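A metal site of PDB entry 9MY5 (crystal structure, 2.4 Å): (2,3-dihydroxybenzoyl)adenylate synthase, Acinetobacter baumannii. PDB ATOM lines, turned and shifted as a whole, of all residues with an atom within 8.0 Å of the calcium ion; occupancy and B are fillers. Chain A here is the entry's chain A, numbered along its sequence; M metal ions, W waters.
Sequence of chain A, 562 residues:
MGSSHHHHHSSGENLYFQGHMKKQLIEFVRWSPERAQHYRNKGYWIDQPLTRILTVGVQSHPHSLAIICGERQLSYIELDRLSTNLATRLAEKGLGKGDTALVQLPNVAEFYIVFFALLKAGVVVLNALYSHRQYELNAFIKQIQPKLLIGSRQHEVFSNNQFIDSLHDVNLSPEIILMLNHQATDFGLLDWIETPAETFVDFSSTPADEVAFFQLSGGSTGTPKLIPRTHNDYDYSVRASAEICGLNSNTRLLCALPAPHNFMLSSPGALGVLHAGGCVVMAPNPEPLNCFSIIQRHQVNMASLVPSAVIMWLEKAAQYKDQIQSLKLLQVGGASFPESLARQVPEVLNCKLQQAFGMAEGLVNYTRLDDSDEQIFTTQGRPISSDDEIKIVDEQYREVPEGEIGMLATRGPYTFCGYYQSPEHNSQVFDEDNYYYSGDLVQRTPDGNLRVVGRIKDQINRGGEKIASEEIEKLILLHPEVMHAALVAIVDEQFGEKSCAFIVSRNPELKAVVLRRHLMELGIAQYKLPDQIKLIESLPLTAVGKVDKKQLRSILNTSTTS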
ATOM      1  N   VAL A 300     -13.555   9.086 -13.167  1.00  0.00           N
ATOM      2  CA  VAL A 300     -14.184   8.084 -12.311  1.00  0.00           C
ATOM      3  C   VAL A 300     -14.634   6.887 -13.148  1.00  0.00           C
ATOM      4  O   VAL A 300     -15.260   7.053 -14.199  1.00  0.00           O
ATOM      5  CB  VAL A 300     -15.370   8.696 -11.549  1.00  0.00           C
ATOM      6  CG1 VAL A 300     -16.273   7.619 -10.982  1.00  0.00           C
ATOM      7  CG2 VAL A 300     -14.869   9.587 -10.445  1.00  0.00           C
ATOM      8  N   ASN A 301     -14.344   5.681 -12.677  1.00  0.00           N
ATOM      9  CA  ASN A 301     -14.706   4.470 -13.412  1.00  0.00           C
ATOM     10  C   ASN A 301     -15.644   3.556 -12.637  1.00  0.00           C
ATOM     11  O   ASN A 301     -16.034   2.509 -13.172  1.00  0.00           O
ATOM     12  CB  ASN A 301     -13.457   3.672 -13.843  1.00  0.00           C
ATOM     13  CG  ASN A 301     -12.525   3.327 -12.675  1.00  0.00           C
ATOM     14  OD1 ASN A 301     -12.957   2.959 -11.570  1.00  0.00           O
ATOM     15  ND2 ASN A 301     -11.228   3.398 -12.932  1.00  0.00           N
ATOM     16  N   LYS A 321     -23.557  12.238 -22.302  1.00  0.00           N
ATOM     17  CA  LYS A 321     -22.856  10.964 -22.427  1.00  0.00           C
ATOM     18  C   LYS A 321     -21.359  11.137 -22.197  1.00  0.00           C
ATOM     19  O   LYS A 321     -20.720  10.304 -21.530  1.00  0.00           O
ATOM     20  CB  LYS A 321     -23.113  10.358 -23.810  1.00  0.00           C
ATOM     21  CG  LYS A 321     -24.092   9.187 -23.822  1.00  0.00           C
ATOM     22  CD  LYS A 321     -24.182   8.513 -25.192  1.00  0.00           C
ATOM     23  N   ILE A 324     -19.779  11.070 -18.586  1.00  0.00           N
ATOM     24  CA  ILE A 324     -19.785   9.812 -17.829  1.00  0.00           C
ATOM     25  C   ILE A 324     -19.223   8.657 -18.654  1.00  0.00           C
ATOM     26  O   ILE A 324     -19.450   7.493 -18.337  1.00  0.00           O
ATOM     27  CB  ILE A 324     -21.201   9.491 -17.306  1.00  0.00           C
ATOM     28  CG1 ILE A 324     -22.161   9.153 -18.460  1.00  0.00           C
ATOM     29  CG2 ILE A 324     -21.767  10.659 -16.485  1.00  0.00           C
ATOM     30  CD1 ILE A 324     -23.455   8.541 -18.004  1.00  0.00           C
ATOM     31  N   GLN A 325     -18.492   8.951 -19.725  1.00  0.00           N
ATOM     32  CA  GLN A 325     -17.980   7.860 -20.540  1.00  0.00           C
ATOM     33  C   GLN A 325     -16.976   7.001 -19.759  1.00  0.00           C
ATOM     34  O   GLN A 325     -16.852   5.798 -20.050  1.00  0.00           O
ATOM     35  CB  GLN A 325     -17.375   8.396 -21.839  1.00  0.00           C
ATOM     36  CG  GLN A 325     -16.176   9.257 -21.598  1.00  0.00           C
ATOM     37  CD  GLN A 325     -14.866   8.495 -21.740  1.00  0.00           C
ATOM     38  OE1 GLN A 325     -14.812   7.430 -22.381  1.00  0.00           O
ATOM     39  NE2 GLN A 325     -13.833   8.985 -21.063  1.00  0.00           N
ATOM     40  N   SER A 326     -16.278   7.569 -18.763  1.00  0.00           N
ATOM     41  CA  SER A 326     -15.252   6.762 -18.095  1.00  0.00           C
ATOM     42  C   SER A 326     -15.858   5.710 -17.180  1.00  0.00           C
ATOM     43  O   SER A 326     -15.154   4.773 -16.788  1.00  0.00           O
ATOM     44  CB  SER A 326     -14.271   7.631 -17.303  1.00  0.00           C
ATOM     45  OG  SER A 326     -14.899   8.301 -16.219  1.00  0.00           O
ATOM     46  N   LEU A 327     -17.136   5.838 -16.840  1.00  0.00           N
ATOM     47  CA  LEU A 327     -17.780   4.859 -15.972  1.00  0.00           C
ATOM     48  C   LEU A 327     -17.659   3.470 -16.568  1.00  0.00           C
ATOM     49  O   LEU A 327     -17.935   3.259 -17.755  1.00  0.00           O
ATOM     50  CB  LEU A 327     -19.251   5.201 -15.798  1.00  0.00           C
ATOM     51  CG  LEU A 327     -19.642   6.135 -14.655  1.00  0.00           C
ATOM     52  CD1 LEU A 327     -21.162   6.060 -14.498  1.00  0.00           C
ATOM     53  CD2 LEU A 327     -18.897   5.774 -13.344  1.00  0.00           C
ATOM     54  N   LYS A 328     -17.223   2.508 -15.748  1.00  0.00           N
ATOM     55  CA  LYS A 328     -17.150   1.131 -16.202  1.00  0.00           C
ATOM     56  C   LYS A 328     -18.054   0.179 -15.438  1.00  0.00           C
ATOM     57  O   LYS A 328     -18.436  -0.855 -15.992  1.00  0.00           O
ATOM     58  CB  LYS A 328     -15.704   0.633 -16.121  1.00  0.00           C
ATOM     59  CG  LYS A 328     -14.773   1.333 -17.113  1.00  0.00           C
ATOM     60  CD  LYS A 328     -13.433   0.614 -17.202  1.00  0.00           C
ATOM     61  CE  LYS A 328     -12.355   1.504 -17.844  1.00  0.00           C
ATOM     62  NZ  LYS A 328     -11.160   1.643 -16.923  1.00  0.00           N
ATOM     63  N   LEU A 329     -18.428   0.496 -14.202  1.00  0.00           N
ATOM     64  CA  LEU A 329     -19.236  -0.403 -13.409  1.00  0.00           C
ATOM     65  C   LEU A 329     -20.099   0.411 -12.461  1.00  0.00           C
ATOM     66  O   LEU A 329     -19.572   1.222 -11.691  1.00  0.00           O
ATOM     67  CB  LEU A 329     -18.354  -1.381 -12.614  1.00  0.00           C
ATOM     68  CG  LEU A 329     -19.131  -2.381 -11.780  1.00  0.00           C
ATOM     69  CD1 LEU A 329     -20.073  -3.164 -12.669  1.00  0.00           C
ATOM     70  CD2 LEU A 329     -18.164  -3.318 -11.031  1.00  0.00           C
ATOM     71  N   PRO A 346     -26.500  -0.280 -19.132  1.00  0.00           N
ATOM     72  CA  PRO A 346     -25.588  -0.363 -20.287  1.00  0.00           C
ATOM     73  C   PRO A 346     -26.005   0.495 -21.460  1.00  0.00           C
ATOM     74  O   PRO A 346     -25.146   1.089 -22.132  1.00  0.00           O
ATOM     75  CB  PRO A 346     -25.605  -1.850 -20.660  1.00  0.00           C
ATOM     76  CG  PRO A 346     -26.772  -2.439 -19.936  1.00  0.00           C
ATOM     77  CD  PRO A 346     -26.979  -1.605 -18.703  1.00  0.00           C
ATOM     78  N   LEU A 349     -26.160   4.545 -19.780  1.00  0.00           N
ATOM     79  CA  LEU A 349     -24.982   4.922 -19.006  1.00  0.00           C
ATOM     80  C   LEU A 349     -23.682   4.378 -19.590  1.00  0.00           C
ATOM     81  O   LEU A 349     -22.605   4.834 -19.192  1.00  0.00           O
ATOM     82  CB  LEU A 349     -25.147   4.480 -17.553  1.00  0.00           C
ATOM     83  CG  LEU A 349     -26.360   5.089 -16.841  1.00  0.00           C
ATOM     84  CD1 LEU A 349     -26.481   4.644 -15.376  1.00  0.00           C
ATOM     85  CD2 LEU A 349     -26.349   6.614 -16.960  1.00  0.00           C
ATOM     86  N   ASN A 350     -23.750   3.458 -20.547  1.00  0.00           N
ATOM     87  CA  ASN A 350     -22.557   2.928 -21.211  1.00  0.00           C
ATOM     88  C   ASN A 350     -21.547   2.425 -20.186  1.00  0.00           C
ATOM     89  O   ASN A 350     -20.367   2.789 -20.200  1.00  0.00           O
ATOM     90  CB  ASN A 350     -21.962   3.977 -22.147  1.00  0.00           C
ATOM     91  CG  ASN A 350     -22.939   4.398 -23.223  1.00  0.00           C
ATOM     92  OD1 ASN A 350     -23.531   3.552 -23.904  1.00  0.00           O
ATOM     93  ND2 ASN A 350     -23.128   5.709 -23.383  1.00  0.00           N
ATOM     94  N   CYS A 351     -22.048   1.600 -19.273  1.00  0.00           N
ATOM     95  CA  CYS A 351     -21.219   0.931 -18.286  1.00  0.00           C
ATOM     96  C   CYS A 351     -21.936  -0.339 -17.875  1.00  0.00           C
ATOM     97  O   CYS A 351     -23.159  -0.430 -17.990  1.00  0.00           O
ATOM     98  CB  CYS A 351     -20.970   1.819 -17.069  1.00  0.00           C
ATOM     99  SG  CYS A 351     -22.444   2.030 -16.067  1.00  0.00           S
ATOM    100  N   LYS A 352     -21.179  -1.311 -17.386  1.00  0.00           N
ATOM    101  CA  LYS A 352     -21.826  -2.541 -16.955  1.00  0.00           C
ATOM    102  C   LYS A 352     -22.523  -2.312 -15.615  1.00  0.00           C
ATOM    103  O   LYS A 352     -22.243  -1.354 -14.885  1.00  0.00           O
ATOM    104  CB  LYS A 352     -20.832  -3.701 -16.841  1.00  0.00           C
ATOM    105  CG  LYS A 352     -21.562  -5.070 -16.825  1.00  0.00           C
ATOM    106  CD  LYS A 352     -22.619  -5.094 -17.943  1.00  0.00           C
ATOM    107  CE  LYS A 352     -23.740  -6.118 -17.695  1.00  0.00           C
ATOM    108  NZ  LYS A 352     -25.052  -5.582 -18.189  1.00  0.00           N
HETATM  109 CA    CA M   1     -18.379   3.839 -19.967  1.00  0.00          CA
HETATM  110  O   HOH W   1     -18.378   1.600 -20.498  1.00  0.00           O
HETATM  111  O   HOH W   2     -15.974   2.689 -20.778  1.00  0.00           O
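Of the 14 residues printed, 3 come within 4 Å of the calcium ion.
The nearest printed residue that does not touch the calcium ion is Ile 324 (4.1 Å).
N of Leu 327 is in hydrogen-bond range of O of Val 300, 3.5 Å away.
O of Pro 346 sits close to OD1 of Asn 350 (3.4 Å).
The calcium ion is bound by O of Asn 350 (2.3 Å), water W1 (2.3 Å), O of Leu 327 (2.3 Å), O of Gln 325 (2.5 Å) and water W2 (2.8 Å).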
